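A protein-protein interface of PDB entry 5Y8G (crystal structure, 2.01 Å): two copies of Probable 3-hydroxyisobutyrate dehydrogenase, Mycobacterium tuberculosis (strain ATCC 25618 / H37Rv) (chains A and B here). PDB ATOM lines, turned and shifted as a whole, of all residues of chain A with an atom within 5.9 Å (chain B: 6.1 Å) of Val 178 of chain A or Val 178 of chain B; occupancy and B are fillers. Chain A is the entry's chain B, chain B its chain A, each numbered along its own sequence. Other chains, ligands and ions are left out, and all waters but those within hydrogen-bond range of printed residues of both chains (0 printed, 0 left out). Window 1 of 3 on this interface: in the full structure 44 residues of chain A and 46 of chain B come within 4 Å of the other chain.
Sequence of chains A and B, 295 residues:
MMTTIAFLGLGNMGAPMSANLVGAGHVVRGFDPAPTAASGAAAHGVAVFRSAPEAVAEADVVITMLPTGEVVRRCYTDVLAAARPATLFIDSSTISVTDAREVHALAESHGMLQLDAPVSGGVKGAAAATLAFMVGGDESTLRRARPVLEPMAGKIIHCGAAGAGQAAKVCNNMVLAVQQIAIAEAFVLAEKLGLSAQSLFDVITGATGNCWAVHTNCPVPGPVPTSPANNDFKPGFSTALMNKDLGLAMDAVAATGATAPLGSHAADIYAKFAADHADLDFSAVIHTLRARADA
OE2 of Glu 185 of chain B lies within hydrogen-bond range of N of Leu 262 of chain A (2.7 Å).
N of Gly 263 of chain A lies within hydrogen-bond range of OE1 of Glu 185 of chain B (2.8 Å).
OE2 of Glu 185 of chain A is in hydrogen-bond range of N of Leu 262 of chain B (2.6 Å).
The backbone NH (N) of Gly 263 of chain B lies within hydrogen-bond range of the side-chain carboxylate (OE1) of Glu 185 of chain A (2.8 Å).
Val 175 of chain A touches Ala 182 of chain B (CG2 to O, 3.9 Å).
Val 178 of chain B touches Val 178 of chain A (CG1 to CG1, 3.4 Å).
CG1 of Val 178 of chain A touches CB of Ala 182 of chain B (3.7 Å).
Val 178 of chain A touches Leu 262 of chain B.
CG of Gln 179 of chain A touches CG of Gln 179 of chain B, at 3.98 Å.
CG2 of Ile 181 of chain A touches CD1 of Leu 262 of chain B, at 3.7 Å.
Val 175 of chain B touches Ala 182 of chain A.
Ala 182 of chain A touches Val 178 of chain B.
Leu 262 of chain A touches Val 178 of chain B (CD1 to O, 3.8 Å).
Leu 262 of chain A touches Ile 181 of chain B (CD1 to CG2, 3.7 Å).
Of the 16 printed residues of chain A, 9 touch a printed residue of chain B.
Printed residues of chain A that touch a printed residue of chain B: Val 175, Val 178, Gln 179, Ile 181, Ala 182, Ile 183, Glu 185, Leu 262 and Gly 263.
Val 178 of chain A touches Ala 182 of chain B, and with the chains exchanged Ala 182 of chain A touches Val 178 of chain B.
Val 178 of chain A touches Leu 262 of chain B, and with the chains exchanged Leu 262 of chain A touches Val 178 of chain B.
Glu 185 of chain A touches Leu 262 of chain B, and with the chains exchanged Leu 262 of chain A touches Glu 185 of chain B.
Glu 185 of chain A touches Gly 263 of chain B, and with the chains exchanged Gly 263 of chain A touches Glu 185 of chain B.
Of the 15 pairs that touch across the chains among the printed residues, 14 have their exchanged pair printed and touching as well.
Of the printed residues of chain B, Val 178 of chain A touches Val 178, Ala 182 and Leu 262.
Of the printed residues of chain A, Val 175 of chain B touches Ala 182 (3.7 Å) and Ile 183 (3.8 Å).
Of chain A, only Val 178 (3.4 Å), Ala 182 (3.7 Å) and Leu 262 (3.8 Å) come within 4 Å of Val 178 of chain B.
Printed residues of chain A within 4 Å of Ile 181 of chain B: Leu 262 (3.7 Å).
The nearest printed residue of chain A that does not touch Val 175 of chain B is Gln 179 of chain A (5.8 Å).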
ATOM      1  N   ASN A 173       2.085  24.371  37.015  1.00  0.00           N
ATOM      2  CA  ASN A 173       3.275  23.712  36.409  1.00  0.00           C
ATOM      3  C   ASN A 173       2.937  22.825  35.191  1.00  0.00           C
ATOM      4  O   ASN A 173       3.750  22.650  34.317  1.00  0.00           O
ATOM      5  CB  ASN A 173       4.159  22.998  37.483  1.00  0.00           C
ATOM      6  CG  ASN A 173       5.033  24.010  38.290  1.00  0.00           C
ATOM      7  OD1 ASN A 173       4.841  25.243  38.202  1.00  0.00           O
ATOM      8  ND2 ASN A 173       5.981  23.521  39.055  1.00  0.00           N
ATOM      9  N   MET A 174       1.748  22.241  35.193  1.00  0.00           N
ATOM     10  CA  MET A 174       1.263  21.495  34.041  1.00  0.00           C
ATOM     11  C   MET A 174       1.130  22.443  32.822  1.00  0.00           C
ATOM     12  O   MET A 174       1.635  22.144  31.765  1.00  0.00           O
ATOM     13  CB  MET A 174      -0.087  20.835  34.337  1.00  0.00           C
ATOM     14  CG  MET A 174      -0.550  19.843  33.257  1.00  0.00           C
ATOM     15  SD  MET A 174      -2.082  18.929  33.703  1.00  0.00           S
ATOM     16  CE  MET A 174      -3.327  20.210  33.681  1.00  0.00           C
ATOM     17  N   VAL A 175       0.461  23.547  33.018  1.00  0.00           N
ATOM     18  CA  VAL A 175       0.351  24.585  32.009  1.00  0.00           C
ATOM     19  C   VAL A 175       1.738  25.029  31.498  1.00  0.00           C
ATOM     20  O   VAL A 175       1.980  25.086  30.280  1.00  0.00           O
ATOM     21  CB  VAL A 175      -0.387  25.787  32.539  1.00  0.00           C
ATOM     22  CG1 VAL A 175      -0.329  26.939  31.544  1.00  0.00           C
ATOM     23  CG2 VAL A 175      -1.825  25.417  32.799  1.00  0.00           C
ATOM     24  N   LEU A 176       2.650  25.289  32.431  1.00  0.00           N
ATOM     25  CA  LEU A 176       4.007  25.618  32.043  1.00  0.00           C
ATOM     26  C   LEU A 176       4.715  24.605  31.161  1.00  0.00           C
ATOM     27  O   LEU A 176       5.316  24.982  30.162  1.00  0.00           O
ATOM     28  CB  LEU A 176       4.833  25.894  33.260  1.00  0.00           C
ATOM     29  CG  LEU A 176       6.311  26.200  33.035  1.00  0.00           C
ATOM     30  CD1 LEU A 176       6.434  27.505  32.268  1.00  0.00           C
ATOM     31  CD2 LEU A 176       6.996  26.261  34.412  1.00  0.00           C
ATOM     32  N   ALA A 177       4.590  23.326  31.480  1.00  0.00           N
ATOM     33  CA  ALA A 177       5.165  22.281  30.723  1.00  0.00           C
ATOM     34  C   ALA A 177       4.611  22.236  29.319  1.00  0.00           C
ATOM     35  O   ALA A 177       5.365  22.089  28.382  1.00  0.00           O
ATOM     36  CB  ALA A 177       4.982  20.930  31.401  1.00  0.00           C
ATOM     37  N   VAL A 178       3.311  22.383  29.176  1.00  0.00           N
ATOM     38  CA  VAL A 178       2.703  22.397  27.864  1.00  0.00           C
ATOM     39  C   VAL A 178       3.208  23.615  27.066  1.00  0.00           C
ATOM     40  O   VAL A 178       3.550  23.519  25.865  1.00  0.00           O
ATOM     41  CB  VAL A 178       1.176  22.429  28.066  1.00  0.00           C
ATOM     42  CG1 VAL A 178       0.452  22.704  26.781  1.00  0.00           C
ATOM     43  CG2 VAL A 178       0.638  21.135  28.673  1.00  0.00           C
ATOM     44  N   GLN A 179       3.256  24.763  27.718  1.00  0.00           N
ATOM     45  CA  GLN A 179       3.714  25.994  27.062  1.00  0.00           C
ATOM     46  C   GLN A 179       5.165  25.934  26.605  1.00  0.00           C
ATOM     47  O   GLN A 179       5.518  26.481  25.575  1.00  0.00           O
ATOM     48  CB  GLN A 179       3.556  27.190  28.000  1.00  0.00           C
ATOM     49  CG  GLN A 179       2.121  27.685  28.221  1.00  0.00           C
ATOM     50  CD  GLN A 179       1.979  28.585  29.439  1.00  0.00           C
ATOM     51  OE1 GLN A 179       2.839  28.589  30.335  1.00  0.00           O
ATOM     52  NE2 GLN A 179       0.892  29.340  29.495  1.00  0.00           N
ATOM     53  N   GLN A 180       6.021  25.323  27.405  1.00  0.00           N
ATOM     54  CA  GLN A 180       7.445  25.219  27.092  1.00  0.00           C
ATOM     55  C   GLN A 180       7.674  24.335  25.857  1.00  0.00           C
ATOM     56  O   GLN A 180       8.522  24.657  24.965  1.00  0.00           O
ATOM     57  CB  GLN A 180       8.271  24.730  28.268  1.00  0.00           C
ATOM     58  CG  GLN A 180       9.773  24.879  28.101  1.00  0.00           C
ATOM     59  CD  GLN A 180      10.266  26.326  28.130  1.00  0.00           C
ATOM     60  OE1 GLN A 180      10.111  27.040  29.128  1.00  0.00           O
ATOM     61  NE2 GLN A 180      10.720  26.813  26.969  1.00  0.00           N
ATOM     62  N   ILE A 181       6.900  23.285  25.763  1.00  0.00           N
ATOM     63  CA  ILE A 181       6.897  22.420  24.556  1.00  0.00           C
ATOM     64  C   ILE A 181       6.353  23.166  23.303  1.00  0.00           C
ATOM     65  O   ILE A 181       6.988  23.133  22.210  1.00  0.00           O
ATOM     66  CB  ILE A 181       6.128  21.120  24.799  1.00  0.00           C
ATOM     67  CG1 ILE A 181       6.893  20.210  25.798  1.00  0.00           C
ATOM     68  CG2 ILE A 181       6.062  20.301  23.488  1.00  0.00           C
ATOM     69  CD1 ILE A 181       6.083  19.082  26.424  1.00  0.00           C
ATOM     70  N   ALA A 182       5.230  23.849  23.480  1.00  0.00           N
ATOM     71  CA  ALA A 182       4.622  24.572  22.399  1.00  0.00           C
ATOM     72  C   ALA A 182       5.496  25.656  21.854  1.00  0.00           C
ATOM     73  O   ALA A 182       5.538  25.808  20.656  1.00  0.00           O
ATOM     74  CB  ALA A 182       3.221  25.120  22.740  1.00  0.00           C
ATOM     75  N   ILE A 183       6.202  26.367  22.731  1.00  0.00           N
ATOM     76  CA  ILE A 183       7.173  27.376  22.340  1.00  0.00           C
ATOM     77  C   ILE A 183       8.317  26.745  21.574  1.00  0.00           C
ATOM     78  O   ILE A 183       8.764  27.300  20.554  1.00  0.00           O
ATOM     79  CB  ILE A 183       7.633  28.216  23.538  1.00  0.00           C
ATOM     80  CG1 ILE A 183       6.457  29.092  24.046  1.00  0.00           C
ATOM     81  CG2 ILE A 183       8.864  29.055  23.256  1.00  0.00           C
ATOM     82  CD1 ILE A 183       5.917  30.175  23.119  1.00  0.00           C
ATOM     83  N   GLU A 185       8.201  23.920  19.800  1.00  0.00           N
ATOM     84  CA  GLU A 185       7.641  23.550  18.525  1.00  0.00           C
ATOM     85  C   GLU A 185       7.542  24.749  17.565  1.00  0.00           C
ATOM     86  O   GLU A 185       7.888  24.636  16.388  1.00  0.00           O
ATOM     87  CB  GLU A 185       6.254  22.977  18.698  1.00  0.00           C
ATOM     88  CG  GLU A 185       6.169  21.639  19.438  1.00  0.00           C
ATOM     89  CD  GLU A 185       4.709  21.160  19.637  1.00  0.00           C
ATOM     90  OE1 GLU A 185       3.702  21.775  19.100  1.00  0.00           O
ATOM     91  OE2 GLU A 185       4.582  20.106  20.308  1.00  0.00           O
ATOM     92  N   LEU A 262      -3.547  17.595  26.671  1.00  0.00           N
ATOM     93  CA  LEU A 262      -2.251  18.121  26.387  1.00  0.00           C
ATOM     94  C   LEU A 262      -1.340  18.011  27.576  1.00  0.00           C
ATOM     95  O   LEU A 262      -0.158  17.773  27.408  1.00  0.00           O
ATOM     96  CB  LEU A 262      -2.298  19.552  25.872  1.00  0.00           C
ATOM     97  CG  LEU A 262      -3.187  19.789  24.651  1.00  0.00           C
ATOM     98  CD1 LEU A 262      -2.941  21.218  24.110  1.00  0.00           C
ATOM     99  CD2 LEU A 262      -2.897  18.797  23.549  1.00  0.00           C
ATOM    100  N   GLY A 263      -1.884  18.151  28.775  1.00  0.00           N
ATOM    101  CA  GLY A 263      -1.075  17.960  30.001  1.00  0.00           C
ATOM    102  C   GLY A 263      -0.533  16.556  30.109  1.00  0.00           C
ATOM    103  O   GLY A 263       0.641  16.346  30.368  1.00  0.00           O
ATOM    104  N   ALA A 266       2.096  16.165  27.419  1.00  0.00           N
ATOM    105  CA  ALA A 266       3.293  16.783  27.881  1.00  0.00           C
ATOM    106  C   ALA A 266       4.018  15.922  28.943  1.00  0.00           C
ATOM    107  O   ALA A 266       5.230  15.835  28.942  1.00  0.00           O
ATOM    108  CB  ALA A 266       2.964  18.155  28.421  1.00  0.00           C
ATOM    109  N   TYR A 270       7.918  14.639  28.558  1.00  0.00           N
ATOM    110  CA  TYR A 270       8.929  14.917  29.614  1.00  0.00           C
ATOM    111  C   TYR A 270       9.464  13.665  30.311  1.00  0.00           C
ATOM    112  O   TYR A 270      10.679  13.624  30.659  1.00  0.00           O
ATOM    113  CB  TYR A 270       8.461  15.945  30.628  1.00  0.00           C
ATOM    114  CG  TYR A 270       8.806  17.372  30.140  1.00  0.00           C
ATOM    115  CD1 TYR A 270      10.141  17.777  30.039  1.00  0.00           C
ATOM    116  CD2 TYR A 270       7.789  18.265  29.757  1.00  0.00           C
ATOM    117  CE1 TYR A 270      10.469  19.021  29.573  1.00  0.00           C
ATOM    118  CE2 TYR A 270       8.085  19.536  29.292  1.00  0.00           C
ATOM    119  CZ  TYR A 270       9.431  19.903  29.202  1.00  0.00           C
ATOM    120  OH  TYR A 270       9.750  21.126  28.744  1.00  0.00           O
ATOM    121  N   ASN B 173      -0.446  31.609  16.403  1.00  0.00           N
ATOM    122  CA  ASN B 173      -1.753  31.032  16.624  1.00  0.00           C
ATOM    123  C   ASN B 173      -1.744  29.533  17.041  1.00  0.00           C
ATOM    124  O   ASN B 173      -2.638  29.105  17.762  1.00  0.00           O
ATOM    125  CB  ASN B 173      -2.701  31.314  15.448  1.00  0.00           C
ATOM    126  CG  ASN B 173      -3.198  32.765  15.461  1.00  0.00           C
ATOM    127  OD1 ASN B 173      -2.723  33.590  16.238  1.00  0.00           O
ATOM    128  ND2 ASN B 173      -4.107  33.080  14.599  1.00  0.00           N
ATOM    129  N   MET B 174      -0.721  28.792  16.606  1.00  0.00           N
ATOM    130  CA  MET B 174      -0.573  27.401  17.025  1.00  0.00           C
ATOM    131  C   MET B 174      -0.258  27.386  18.553  1.00  0.00           C
ATOM    132  O   MET B 174      -0.875  26.612  19.313  1.00  0.00           O
ATOM    133  CB  MET B 174       0.533  26.692  16.256  1.00  0.00           C
ATOM    134  CG  MET B 174       0.677  25.217  16.616  1.00  0.00           C
ATOM    135  SD  MET B 174       1.871  24.368  15.539  1.00  0.00           S
ATOM    136  CE  MET B 174       3.446  25.098  16.048  1.00  0.00           C
ATOM    137  N   VAL B 175       0.646  28.274  18.999  1.00  0.00           N
ATOM    138  CA  VAL B 175       0.938  28.402  20.436  1.00  0.00           C
ATOM    139  C   VAL B 175      -0.333  28.731  21.223  1.00  0.00           C
ATOM    140  O   VAL B 175      -0.621  28.108  22.277  1.00  0.00           O
ATOM    141  CB  VAL B 175       2.075  29.400  20.676  1.00  0.00           C
ATOM    142  CG1 VAL B 175       2.240  29.785  22.151  1.00  0.00           C
ATOM    143  CG2 VAL B 175       3.364  28.793  20.166  1.00  0.00           C
ATOM    144  N   LEU B 176      -1.042  29.744  20.736  1.00  0.00           N
ATOM    145  CA  LEU B 176      -2.294  30.239  21.335  1.00  0.00           C
ATOM    146  C   LEU B 176      -3.314  29.138  21.539  1.00  0.00           C
ATOM    147  O   LEU B 176      -3.907  29.036  22.577  1.00  0.00           O
ATOM    148  CB  LEU B 176      -2.905  31.340  20.487  1.00  0.00           C
ATOM    149  CG  LEU B 176      -4.212  31.939  20.984  1.00  0.00           C
ATOM    150  CD1 LEU B 176      -4.175  32.453  22.431  1.00  0.00           C
ATOM    151  CD2 LEU B 176      -4.671  33.076  20.088  1.00  0.00           C
ATOM    152  N   ALA B 177      -3.474  28.302  20.512  1.00  0.00           N
ATOM    153  CA  ALA B 177      -4.416  27.241  20.573  1.00  0.00           C
ATOM    154  C   ALA B 177      -4.071  26.245  21.671  1.00  0.00           C
ATOM    155  O   ALA B 177      -4.999  25.791  22.397  1.00  0.00           O
ATOM    156  CB  ALA B 177      -4.542  26.546  19.224  1.00  0.00           C
ATOM    157  N   VAL B 178      -2.789  25.878  21.750  1.00  0.00           N
ATOM    158  CA  VAL B 178      -2.286  24.950  22.732  1.00  0.00           C
ATOM    159  C   VAL B 178      -2.546  25.577  24.121  1.00  0.00           C
ATOM    160  O   VAL B 178      -3.053  24.912  24.995  1.00  0.00           O
ATOM    161  CB  VAL B 178      -0.782  24.649  22.518  1.00  0.00           C
ATOM    162  CG1 VAL B 178      -0.139  23.946  23.717  1.00  0.00           C
ATOM    163  CG2 VAL B 178      -0.565  23.791  21.276  1.00  0.00           C
ATOM    164  N   GLN B 179      -2.226  26.858  24.293  1.00  0.00           N
ATOM    165  CA  GLN B 179      -2.390  27.564  25.572  1.00  0.00           C
ATOM    166  C   GLN B 179      -3.880  27.584  26.006  1.00  0.00           C
ATOM    167  O   GLN B 179      -4.177  27.453  27.206  1.00  0.00           O
ATOM    168  CB  GLN B 179      -1.854  29.000  25.527  1.00  0.00           C
ATOM    169  CG  GLN B 179      -0.327  29.130  25.435  1.00  0.00           C
ATOM    170  CD  GLN B 179       0.153  30.494  25.021  1.00  0.00           C
ATOM    171  OE1 GLN B 179      -0.605  31.266  24.357  1.00  0.00           O
ATOM    172  NE2 GLN B 179       1.423  30.848  25.432  1.00  0.00           N
ATOM    173  N   GLN B 180      -4.791  27.800  25.045  1.00  0.00           N
ATOM    174  CA  GLN B 180      -6.222  27.911  25.385  1.00  0.00           C
ATOM    175  C   GLN B 180      -6.721  26.578  25.884  1.00  0.00           C
ATOM    176  O   GLN B 180      -7.535  26.536  26.822  1.00  0.00           O
ATOM    177  CB  GLN B 180      -7.052  28.413  24.252  1.00  0.00           C
ATOM    178  CG  GLN B 180      -8.443  28.870  24.698  1.00  0.00           C
ATOM    179  CD  GLN B 180      -8.448  30.196  25.482  1.00  0.00           C
ATOM    180  OE1 GLN B 180      -8.081  31.239  24.986  1.00  0.00           O
ATOM    181  NE2 GLN B 180      -8.851  30.137  26.720  1.00  0.00           N
ATOM    182  N   ILE B 181      -6.217  25.492  25.274  1.00  0.00           N
ATOM    183  CA  ILE B 181      -6.551  24.194  25.752  1.00  0.00           C
ATOM    184  C   ILE B 181      -5.933  23.868  27.082  1.00  0.00           C
ATOM    185  O   ILE B 181      -6.619  23.384  28.018  1.00  0.00           O
ATOM    186  CB  ILE B 181      -6.201  23.095  24.725  1.00  0.00           C
ATOM    187  CG1 ILE B 181      -7.107  23.272  23.496  1.00  0.00           C
ATOM    188  CG2 ILE B 181      -6.420  21.705  25.318  1.00  0.00           C
ATOM    189  CD1 ILE B 181      -6.557  22.604  22.277  1.00  0.00           C
ATOM    190  N   ALA B 182      -4.656  24.107  27.201  1.00  0.00           N
ATOM    191  CA  ALA B 182      -4.004  23.872  28.503  1.00  0.00           C
ATOM    192  C   ALA B 182      -4.650  24.623  29.655  1.00  0.00           C
ATOM    193  O   ALA B 182      -4.825  24.036  30.756  1.00  0.00           O
ATOM    194  CB  ALA B 182      -2.520  24.194  28.442  1.00  0.00           C
ATOM    195  N   ILE B 183      -5.002  25.887  29.403  1.00  0.00           N
ATOM    196  CA  ILE B 183      -5.666  26.702  30.417  1.00  0.00           C
ATOM    197  C   ILE B 183      -7.004  26.097  30.808  1.00  0.00           C
ATOM    198  O   ILE B 183      -7.351  26.047  32.026  1.00  0.00           O
ATOM    199  CB  ILE B 183      -5.819  28.170  29.976  1.00  0.00           C
ATOM    200  CG1 ILE B 183      -4.450  28.868  30.077  1.00  0.00           C
ATOM    201  CG2 ILE B 183      -6.861  28.925  30.767  1.00  0.00           C
ATOM    202  CD1 ILE B 183      -3.895  29.067  31.476  1.00  0.00           C
ATOM    203  N   GLU B 185      -7.869  22.894  30.593  1.00  0.00           N
ATOM    204  CA  GLU B 185      -7.611  21.670  31.356  1.00  0.00           C
ATOM    205  C   GLU B 185      -7.289  22.021  32.815  1.00  0.00           C
ATOM    206  O   GLU B 185      -7.740  21.367  33.761  1.00  0.00           O
ATOM    207  CB  GLU B 185      -6.383  20.930  30.814  1.00  0.00           C
ATOM    208  CG  GLU B 185      -6.541  20.363  29.436  1.00  0.00           C
ATOM    209  CD  GLU B 185      -5.204  19.744  28.855  1.00  0.00           C
ATOM    210  OE1 GLU B 185      -4.122  19.600  29.516  1.00  0.00           O
ATOM    211  OE2 GLU B 185      -5.249  19.391  27.674  1.00  0.00           O
ATOM    212  N   LEU B 262       2.313  18.790  20.228  1.00  0.00           N
ATOM    213  CA  LEU B 262       1.192  19.437  20.901  1.00  0.00           C
ATOM    214  C   LEU B 262       0.354  20.320  19.946  1.00  0.00           C
ATOM    215  O   LEU B 262      -0.879  20.372  20.048  1.00  0.00           O
ATOM    216  CB  LEU B 262       1.643  20.224  22.130  1.00  0.00           C
ATOM    217  CG  LEU B 262       2.310  19.387  23.249  1.00  0.00           C
ATOM    218  CD1 LEU B 262       2.466  20.293  24.492  1.00  0.00           C
ATOM    219  CD2 LEU B 262       1.617  18.096  23.630  1.00  0.00           C
ATOM    220  N   GLY B 263       1.008  21.027  19.044  1.00  0.00           N
ATOM    221  CA  GLY B 263       0.243  21.752  18.072  1.00  0.00           C
ATOM    222  C   GLY B 263      -0.674  20.851  17.257  1.00  0.00           C
ATOM    223  O   GLY B 263      -1.818  21.195  17.046  1.00  0.00           O
ATOM    224  N   SER B 264      -0.159  19.731  16.782  1.00  0.00           N
ATOM    225  CA  SER B 264      -0.954  18.761  16.014  1.00  0.00           C
ATOM    226  C   SER B 264      -2.062  18.189  16.822  1.00  0.00           C
ATOM    227  O   SER B 264      -3.141  17.978  16.315  1.00  0.00           O
ATOM    228  CB  SER B 264      -0.114  17.628  15.474  1.00  0.00           C
ATOM    229  OG  SER B 264       0.932  18.152  14.709  1.00  0.00           O
ATOM    230  N   ALA B 266      -3.545  19.767  19.311  1.00  0.00           N
ATOM    231  CA  ALA B 266      -4.460  20.862  19.450  1.00  0.00           C
ATOM    232  C   ALA B 266      -5.334  21.010  18.189  1.00  0.00           C
ATOM    233  O   ALA B 266      -6.552  21.265  18.249  1.00  0.00           O
ATOM    234  CB  ALA B 266      -3.678  22.130  19.721  1.00  0.00           C
ATOM    235  N   TYR B 270      -9.360  20.900  17.981  1.00  0.00           N
ATOM    236  CA  TYR B 270     -10.200  21.994  17.487  1.00  0.00           C
ATOM    237  C   TYR B 270     -11.018  21.608  16.222  1.00  0.00           C
ATOM    238  O   TYR B 270     -12.087  22.166  16.026  1.00  0.00           O
ATOM    239  CB  TYR B 270      -9.385  23.294  17.264  1.00  0.00           C
ATOM    240  CG  TYR B 270      -9.311  24.177  18.519  1.00  0.00           C
ATOM    241  CD1 TYR B 270     -10.455  24.761  19.026  1.00  0.00           C
ATOM    242  CD2 TYR B 270      -8.121  24.333  19.232  1.00  0.00           C
ATOM    243  CE1 TYR B 270     -10.446  25.533  20.202  1.00  0.00           C
ATOM    244  CE2 TYR B 270      -8.090  25.111  20.402  1.00  0.00           C
ATOM    245  CZ  TYR B 270      -9.240  25.719  20.874  1.00  0.00           C
ATOM    246  OH  TYR B 270      -9.284  26.468  22.037  1.00  0.00           O
